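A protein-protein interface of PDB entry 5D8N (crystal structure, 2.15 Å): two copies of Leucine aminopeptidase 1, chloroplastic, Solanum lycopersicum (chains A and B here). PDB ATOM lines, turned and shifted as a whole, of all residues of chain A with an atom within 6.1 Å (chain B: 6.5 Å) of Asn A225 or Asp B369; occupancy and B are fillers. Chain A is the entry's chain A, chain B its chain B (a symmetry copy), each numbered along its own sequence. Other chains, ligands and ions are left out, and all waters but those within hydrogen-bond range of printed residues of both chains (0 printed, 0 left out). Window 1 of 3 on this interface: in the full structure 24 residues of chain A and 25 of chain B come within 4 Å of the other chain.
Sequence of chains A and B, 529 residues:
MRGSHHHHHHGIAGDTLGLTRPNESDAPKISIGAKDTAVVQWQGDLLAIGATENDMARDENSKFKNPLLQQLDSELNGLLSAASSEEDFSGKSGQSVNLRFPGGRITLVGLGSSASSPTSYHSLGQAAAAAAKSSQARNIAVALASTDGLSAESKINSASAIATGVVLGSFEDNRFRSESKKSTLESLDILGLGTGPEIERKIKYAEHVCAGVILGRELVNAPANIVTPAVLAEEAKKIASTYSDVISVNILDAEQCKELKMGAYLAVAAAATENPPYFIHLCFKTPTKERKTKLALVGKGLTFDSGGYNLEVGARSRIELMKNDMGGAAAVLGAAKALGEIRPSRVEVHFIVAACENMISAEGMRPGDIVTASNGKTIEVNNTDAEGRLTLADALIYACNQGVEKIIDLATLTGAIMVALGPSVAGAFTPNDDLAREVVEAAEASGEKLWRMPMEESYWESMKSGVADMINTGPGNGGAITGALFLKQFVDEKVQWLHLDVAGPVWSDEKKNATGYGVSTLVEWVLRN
O of Ile B370 sits at hydrogen-bond distance from OG1 of Thr A20 (2.6 Å).
The backbone NH (N) of Asn A225 sits at hydrogen-bond distance from the side-chain carboxylate (OD1) of Asp B369 (3.5 Å).
The side-chain amide nitrogen (ND2) of Asn A225 is in hydrogen-bond range of the backbone carbonyl oxygen (O) of Ile B370 (2.9 Å).
The side-chain amide nitrogen of Asn A225 sits at hydrogen-bond distance from the backbone carbonyl oxygen of Leu A17 (2.9 Å).
The side-chain hydroxyl (OG1) of Thr A20 sits at hydrogen-bond distance from the backbone carbonyl oxygen (O) of Gly A18 (3.5 Å).
The guanidinium group of Arg B366 lies within salt-bridge range of the side-chain carboxylate of Asp B369 (2.9 Å).
The backbone carbonyl oxygen (O) of Val B381 is in hydrogen-bond range of the backbone NH (N) of Gly B368 (2.7 Å).
The backbone NH (N) of Val B381 lies within hydrogen-bond range of the backbone carbonyl oxygen (O) of Asp B369.
The backbone NH (N) of Ile B379 is in hydrogen-bond range of the backbone carbonyl oxygen (O) of Val B371 (2.8 Å).
Leu A17 touches Met B365.
Leu A17 touches Arg B366 (CD1 to NH2, 3.995 Å).
Leu A17 touches Asp B369.
Val B371 touches Gly A18 (C to O, 3.8 Å).
Thr A20 touches Val B371.
CB of Pro A223 touches O of Gly B368 (3.4 Å).
Pro A223 touches Ile B370 (CG to CD1, 3.8 Å).
Arg B366 touches Ala A224 (NE to CB, 3.6 Å).
Ala A224 touches Asp B369.
Phe A304 touches Arg B366 (CG to CD, 3.6 Å).
Printed residues of chain A within 4 Å of Asp B369: Leu A17 (3.6 Å), Ala A224 (3.99 Å) and Asn A225 (3.4 Å).
Printed residues of chain B within 4 Å of Thr A20: Ile B370 (2.6 Å) and Val B371 (3.3 Å).
Of the printed residues of chain A, Gly B368 touches Pro A223 (3.4 Å).
Of the printed residues of chain A, Gly B364 touches Leu A17 (3.8 Å).
Of the printed residues of chain B, Pro A223 touches Gly B368 (3.4 Å) and Ile B370 (3.8 Å).
Printed residues of chain A within 4 Å of Arg B366: Leu A17, Ala A224, Asn A225 and Phe A304.
Val A227 touches none of the printed residues of chain B.
The nearest residue of chain B that does not touch Asn A225 is Val B371 (4.8 Å).
The nearest printed residue of chain A that does not touch Gly B368 is Asn A225 (5.0 Å).
Of the 12 printed residues of chain B, 8 touch a printed residue of chain A.
Among the printed residues, no Asp or Glu carboxylate lies within 4 Å of a Lys or Arg side-chain nitrogen of the other chain.
No position is printed for both chains.
Of the 16 pairs that touch across the chains among the printed residues, none has its exchanged pair printed and touching as well.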
ATOM      1  N   THR A  16     -33.478  17.514  11.775  1.00  0.00           N
ATOM      2  CA  THR A  16     -32.268  16.975  11.196  1.00  0.00           C
ATOM      3  C   THR A  16     -32.305  15.447  11.090  1.00  0.00           C
ATOM      4  O   THR A  16     -32.603  14.736  12.051  1.00  0.00           O
ATOM      5  CB  THR A  16     -31.087  17.438  12.054  1.00  0.00           C
ATOM      6  OG1 THR A  16     -31.051  18.869  12.017  1.00  0.00           O
ATOM      7  CG2 THR A  16     -29.764  16.906  11.537  1.00  0.00           C
ATOM      8  N   LEU A  17     -31.974  14.930   9.916  1.00  0.00           N
ATOM      9  CA  LEU A  17     -31.813  13.486   9.740  1.00  0.00           C
ATOM     10  C   LEU A  17     -30.743  12.919  10.669  1.00  0.00           C
ATOM     11  O   LEU A  17     -29.684  13.506  10.839  1.00  0.00           O
ATOM     12  CB  LEU A  17     -31.472  13.149   8.287  1.00  0.00           C
ATOM     13  CG  LEU A  17     -31.296  11.654   7.975  1.00  0.00           C
ATOM     14  CD1 LEU A  17     -31.762  11.340   6.558  1.00  0.00           C
ATOM     15  CD2 LEU A  17     -29.857  11.218   8.159  1.00  0.00           C
ATOM     16  N   GLY A  18     -31.094  11.876  11.412  1.00  0.00           N
ATOM     17  CA  GLY A  18     -30.207  11.320  12.436  1.00  0.00           C
ATOM     18  C   GLY A  18     -30.193  12.034  13.775  1.00  0.00           C
ATOM     19  O   GLY A  18     -29.441  11.660  14.671  1.00  0.00           O
ATOM     20  N   LEU A  19     -30.988  13.089  13.884  1.00  0.00           N
ATOM     21  CA  LEU A  19     -31.181  13.837  15.124  1.00  0.00           C
ATOM     22  C   LEU A  19     -29.890  14.448  15.653  1.00  0.00           C
ATOM     23  O   LEU A  19     -29.718  14.598  16.851  1.00  0.00           O
ATOM     24  CB  LEU A  19     -31.833  12.941  16.189  1.00  0.00           C
ATOM     25  CG  LEU A  19     -33.179  12.375  15.764  1.00  0.00           C
ATOM     26  CD1 LEU A  19     -33.738  11.456  16.841  1.00  0.00           C
ATOM     27  CD2 LEU A  19     -34.155  13.505  15.453  1.00  0.00           C
ATOM     28  N   THR A  20     -28.981  14.778  14.746  1.00  0.00           N
ATOM     29  CA  THR A  20     -27.675  15.248  15.115  1.00  0.00           C
ATOM     30  C   THR A  20     -27.724  16.737  15.422  1.00  0.00           C
ATOM     31  O   THR A  20     -28.378  17.517  14.730  1.00  0.00           O
ATOM     32  CB  THR A  20     -26.652  14.887  14.036  1.00  0.00           C
ATOM     33  OG1 THR A  20     -26.535  13.459  14.006  1.00  0.00           O
ATOM     34  CG2 THR A  20     -25.283  15.514  14.320  1.00  0.00           C
ATOM     35  N   PRO A 223     -21.300  17.401   7.600  1.00  0.00           N
ATOM     36  CA  PRO A 223     -21.915  16.486   6.653  1.00  0.00           C
ATOM     37  C   PRO A 223     -23.165  17.082   6.018  1.00  0.00           C
ATOM     38  O   PRO A 223     -23.727  18.087   6.493  1.00  0.00           O
ATOM     39  CB  PRO A 223     -22.267  15.305   7.543  1.00  0.00           C
ATOM     40  CG  PRO A 223     -22.683  15.973   8.824  1.00  0.00           C
ATOM     41  CD  PRO A 223     -21.739  17.125   8.975  1.00  0.00           C
ATOM     42  N   ALA A 224     -23.590  16.440   4.941  1.00  0.00           N
ATOM     43  CA  ALA A 224     -24.708  16.911   4.135  1.00  0.00           C
ATOM     44  C   ALA A 224     -26.048  16.955   4.866  1.00  0.00           C
ATOM     45  O   ALA A 224     -26.950  17.668   4.430  1.00  0.00           O
ATOM     46  CB  ALA A 224     -24.820  16.070   2.883  1.00  0.00           C
ATOM     47  N   ASN A 225     -26.211  16.173   5.932  1.00  0.00           N
ATOM     48  CA  ASN A 225     -27.441  16.214   6.732  1.00  0.00           C
ATOM     49  C   ASN A 225     -27.478  17.426   7.655  1.00  0.00           C
ATOM     50  O   ASN A 225     -28.512  17.767   8.207  1.00  0.00           O
ATOM     51  CB  ASN A 225     -27.699  14.897   7.487  1.00  0.00           C
ATOM     52  CG  ASN A 225     -26.636  14.551   8.506  1.00  0.00           C
ATOM     53  OD1 ASN A 225     -25.441  14.627   8.244  1.00  0.00           O
ATOM     54  ND2 ASN A 225     -27.077  14.139   9.682  1.00  0.00           N
ATOM     55  N   ILE A 226     -26.369  18.139   7.745  1.00  0.00           N
ATOM     56  CA  ILE A 226     -26.277  19.364   8.540  1.00  0.00           C
ATOM     57  C   ILE A 226     -26.136  20.593   7.631  1.00  0.00           C
ATOM     58  O   ILE A 226     -26.897  21.544   7.737  1.00  0.00           O
ATOM     59  CB  ILE A 226     -25.023  19.292   9.458  1.00  0.00           C
ATOM     60  CG1 ILE A 226     -25.145  18.159  10.471  1.00  0.00           C
ATOM     61  CG2 ILE A 226     -24.765  20.622  10.159  1.00  0.00           C
ATOM     62  CD1 ILE A 226     -26.212  18.336  11.530  1.00  0.00           C
ATOM     63  N   VAL A 227     -25.164  20.593   6.723  1.00  0.00           N
ATOM     64  CA  VAL A 227     -25.076  21.652   5.722  1.00  0.00           C
ATOM     65  C   VAL A 227     -25.802  21.258   4.442  1.00  0.00           C
ATOM     66  O   VAL A 227     -25.235  20.592   3.570  1.00  0.00           O
ATOM     67  CB  VAL A 227     -23.619  22.085   5.450  1.00  0.00           C
ATOM     68  CG1 VAL A 227     -23.539  23.086   4.292  1.00  0.00           C
ATOM     69  CG2 VAL A 227     -23.049  22.772   6.687  1.00  0.00           C
ATOM     70  N   THR A 228     -27.100  21.523   4.457  1.00  0.00           N
ATOM     71  CA  THR A 228     -27.978  21.428   3.313  1.00  0.00           C
ATOM     72  C   THR A 228     -27.888  22.708   2.505  1.00  0.00           C
ATOM     73  O   THR A 228     -27.218  23.640   2.912  1.00  0.00           O
ATOM     74  CB  THR A 228     -29.423  21.295   3.798  1.00  0.00           C
ATOM     75  OG1 THR A 228     -29.739  22.422   4.612  1.00  0.00           O
ATOM     76  CG2 THR A 228     -29.598  20.020   4.632  1.00  0.00           C
ATOM     77  N   PHE A 304     -24.133  17.592  -1.261  1.00  0.00           N
ATOM     78  CA  PHE A 304     -23.804  16.180  -1.427  1.00  0.00           C
ATOM     79  C   PHE A 304     -23.845  15.825  -2.912  1.00  0.00           C
ATOM     80  O   PHE A 304     -24.780  16.198  -3.641  1.00  0.00           O
ATOM     81  CB  PHE A 304     -24.808  15.295  -0.670  1.00  0.00           C
ATOM     82  CG  PHE A 304     -24.594  13.824  -0.875  1.00  0.00           C
ATOM     83  CD1 PHE A 304     -23.529  13.171  -0.291  1.00  0.00           C
ATOM     84  CD2 PHE A 304     -25.409  13.111  -1.738  1.00  0.00           C
ATOM     85  CE1 PHE A 304     -23.239  11.856  -0.606  1.00  0.00           C
ATOM     86  CE2 PHE A 304     -25.131  11.789  -2.045  1.00  0.00           C
ATOM     87  CZ  PHE A 304     -24.036  11.160  -1.485  1.00  0.00           C
ATOM     88  N   GLY B 364     -33.754  10.033   1.988  1.00  0.00           N
ATOM     89  CA  GLY B 364     -32.842   9.049   2.567  1.00  0.00           C
ATOM     90  C   GLY B 364     -31.567   9.640   3.147  1.00  0.00           C
ATOM     91  O   GLY B 364     -31.165  10.780   2.841  1.00  0.00           O
ATOM     92  N   MET B 365     -30.897   8.820   3.948  1.00  0.00           N
ATOM     93  CA  MET B 365     -29.574   9.132   4.475  1.00  0.00           C
ATOM     94  C   MET B 365     -28.526   9.010   3.375  1.00  0.00           C
ATOM     95  O   MET B 365     -28.637   8.154   2.529  1.00  0.00           O
ATOM     96  CB  MET B 365     -29.266   8.178   5.622  1.00  0.00           C
ATOM     97  CG  MET B 365     -27.862   8.308   6.184  1.00  0.00           C
ATOM     98  SD  MET B 365     -27.620   7.371   7.701  1.00  0.00           S
ATOM     99  CE  MET B 365     -28.050   5.723   7.141  1.00  0.00           C
ATOM    100  N   ARG B 366     -27.531   9.889   3.364  1.00  0.00           N
ATOM    101  CA  ARG B 366     -26.463   9.839   2.385  1.00  0.00           C
ATOM    102  C   ARG B 366     -25.239   9.214   3.067  1.00  0.00           C
ATOM    103  O   ARG B 366     -25.002   9.455   4.248  1.00  0.00           O
ATOM    104  CB  ARG B 366     -26.105  11.267   1.941  1.00  0.00           C
ATOM    105  CG  ARG B 366     -27.191  12.069   1.209  1.00  0.00           C
ATOM    106  CD  ARG B 366     -27.148  13.553   1.609  1.00  0.00           C
ATOM    107  NE  ARG B 366     -27.601  13.727   2.984  1.00  0.00           N
ATOM    108  CZ  ARG B 366     -28.863  13.948   3.326  1.00  0.00           C
ATOM    109  NH1 ARG B 366     -29.693  14.473   2.430  1.00  0.00           N
ATOM    110  NH2 ARG B 366     -29.257  13.741   4.578  1.00  0.00           N
ATOM    111  N   PRO B 367     -24.315   8.658   2.273  1.00  0.00           N
ATOM    112  CA  PRO B 367     -22.997   8.350   2.809  1.00  0.00           C
ATOM    113  C   PRO B 367     -22.284   9.599   3.267  1.00  0.00           C
ATOM    114  O   PRO B 367     -22.475  10.652   2.669  1.00  0.00           O
ATOM    115  CB  PRO B 367     -22.241   7.735   1.627  1.00  0.00           C
ATOM    116  CG  PRO B 367     -23.038   8.059   0.417  1.00  0.00           C
ATOM    117  CD  PRO B 367     -24.462   8.258   0.863  1.00  0.00           C
ATOM    118  N   GLY B 368     -21.597   9.514   4.403  1.00  0.00           N
ATOM    119  CA  GLY B 368     -21.035  10.689   5.058  1.00  0.00           C
ATOM    120  C   GLY B 368     -21.889  11.384   6.115  1.00  0.00           C
ATOM    121  O   GLY B 368     -21.364  12.130   6.950  1.00  0.00           O
ATOM    122  N   ASP B 369     -23.192  11.132   6.126  1.00  0.00           N
ATOM    123  CA  ASP B 369     -24.058  11.735   7.135  1.00  0.00           C
ATOM    124  C   ASP B 369     -23.590  11.322   8.521  1.00  0.00           C
ATOM    125  O   ASP B 369     -23.056  10.221   8.698  1.00  0.00           O
ATOM    126  CB  ASP B 369     -25.507  11.281   6.952  1.00  0.00           C
ATOM    127  CG  ASP B 369     -26.240  12.042   5.829  1.00  0.00           C
ATOM    128  OD1 ASP B 369     -25.612  12.862   5.118  1.00  0.00           O
ATOM    129  OD2 ASP B 369     -27.411  11.683   5.584  1.00  0.00           O
ATOM    130  N   ILE B 370     -23.820  12.193   9.501  1.00  0.00           N
ATOM    131  CA  ILE B 370     -23.460  11.899  10.867  1.00  0.00           C
ATOM    132  C   ILE B 370     -24.746  11.823  11.666  1.00  0.00           C
ATOM    133  O   ILE B 370     -25.546  12.762  11.667  1.00  0.00           O
ATOM    134  CB  ILE B 370     -22.560  12.977  11.467  1.00  0.00           C
ATOM    135  CG1 ILE B 370     -21.210  13.007  10.779  1.00  0.00           C
ATOM    136  CG2 ILE B 370     -22.366  12.716  12.953  1.00  0.00           C
ATOM    137  CD1 ILE B 370     -20.358  14.196  11.178  1.00  0.00           C
ATOM    138  N   VAL B 371     -25.000  10.652  12.233  1.00  0.00           N
ATOM    139  CA  VAL B 371     -26.251  10.381  12.928  1.00  0.00           C
ATOM    140  C   VAL B 371     -25.950  10.186  14.400  1.00  0.00           C
ATOM    141  O   VAL B 371     -24.827   9.827  14.766  1.00  0.00           O
ATOM    142  CB  VAL B 371     -26.975   9.144  12.370  1.00  0.00           C
ATOM    143  CG1 VAL B 371     -27.131   9.287  10.868  1.00  0.00           C
ATOM    144  CG2 VAL B 371     -26.208   7.859  12.659  1.00  0.00           C
ATOM    145  N   ILE B 379     -22.210   8.804  14.869  1.00  0.00           N
ATOM    146  CA  ILE B 379     -21.677   7.857  13.917  1.00  0.00           C
ATOM    147  C   ILE B 379     -21.602   8.480  12.535  1.00  0.00           C
ATOM    148  O   ILE B 379     -22.592   9.012  12.024  1.00  0.00           O
ATOM    149  CB  ILE B 379     -22.602   6.624  13.839  1.00  0.00           C
ATOM    150  CG1 ILE B 379     -22.794   6.024  15.227  1.00  0.00           C
ATOM    151  CG2 ILE B 379     -22.055   5.575  12.886  1.00  0.00           C
ATOM    152  CD1 ILE B 379     -24.150   5.382  15.368  1.00  0.00           C
ATOM    153  N   GLU B 380     -20.404   8.494  11.973  1.00  0.00           N
ATOM    154  CA  GLU B 380     -20.203   8.909  10.592  1.00  0.00           C
ATOM    155  C   GLU B 380     -20.379   7.741   9.631  1.00  0.00           C
ATOM    156  O   GLU B 380     -19.811   6.670   9.825  1.00  0.00           O
ATOM    157  CB  GLU B 380     -18.799   9.447  10.384  1.00  0.00           C
ATOM    158  CG  GLU B 380     -18.544   9.805   8.933  1.00  0.00           C
ATOM    159  CD  GLU B 380     -17.151  10.328   8.682  1.00  0.00           C
ATOM    160  OE1 GLU B 380     -16.207  10.035   9.462  1.00  0.00           O
ATOM    161  OE2 GLU B 380     -17.037  11.106   7.710  1.00  0.00           O
ATOM    162  N   VAL B 381     -21.384   7.842   8.787  1.00  0.00           N
ATOM    163  CA  VAL B 381     -21.828   6.678   8.066  1.00  0.00           C
ATOM    164  C   VAL B 381     -21.004   6.630   6.788  1.00  0.00           C
ATOM    165  O   VAL B 381     -21.383   7.219   5.800  1.00  0.00           O
ATOM    166  CB  VAL B 381     -23.336   6.727   7.766  1.00  0.00           C
ATOM    167  CG1 VAL B 381     -23.756   5.531   6.923  1.00  0.00           C
ATOM    168  CG2 VAL B 381     -24.151   6.746   9.060  1.00  0.00           C
ATOM    169  N   ASN B 382     -19.862   5.955   6.821  1.00  0.00           N
ATOM    170  CA  ASN B 382     -18.947   5.968   5.688  1.00  0.00           C
ATOM    171  C   ASN B 382     -19.325   4.900   4.692  1.00  0.00           C
ATOM    172  O   ASN B 382     -18.877   4.949   3.555  1.00  0.00           O
ATOM    173  CB  ASN B 382     -17.504   5.747   6.121  1.00  0.00           C
ATOM    174  CG  ASN B 382     -17.294   4.409   6.817  1.00  0.00           C
ATOM    175  OD1 ASN B 382     -18.040   4.039   7.711  1.00  0.00           O
ATOM    176  ND2 ASN B 382     -16.185   3.755   6.520  1.00  0.00           N
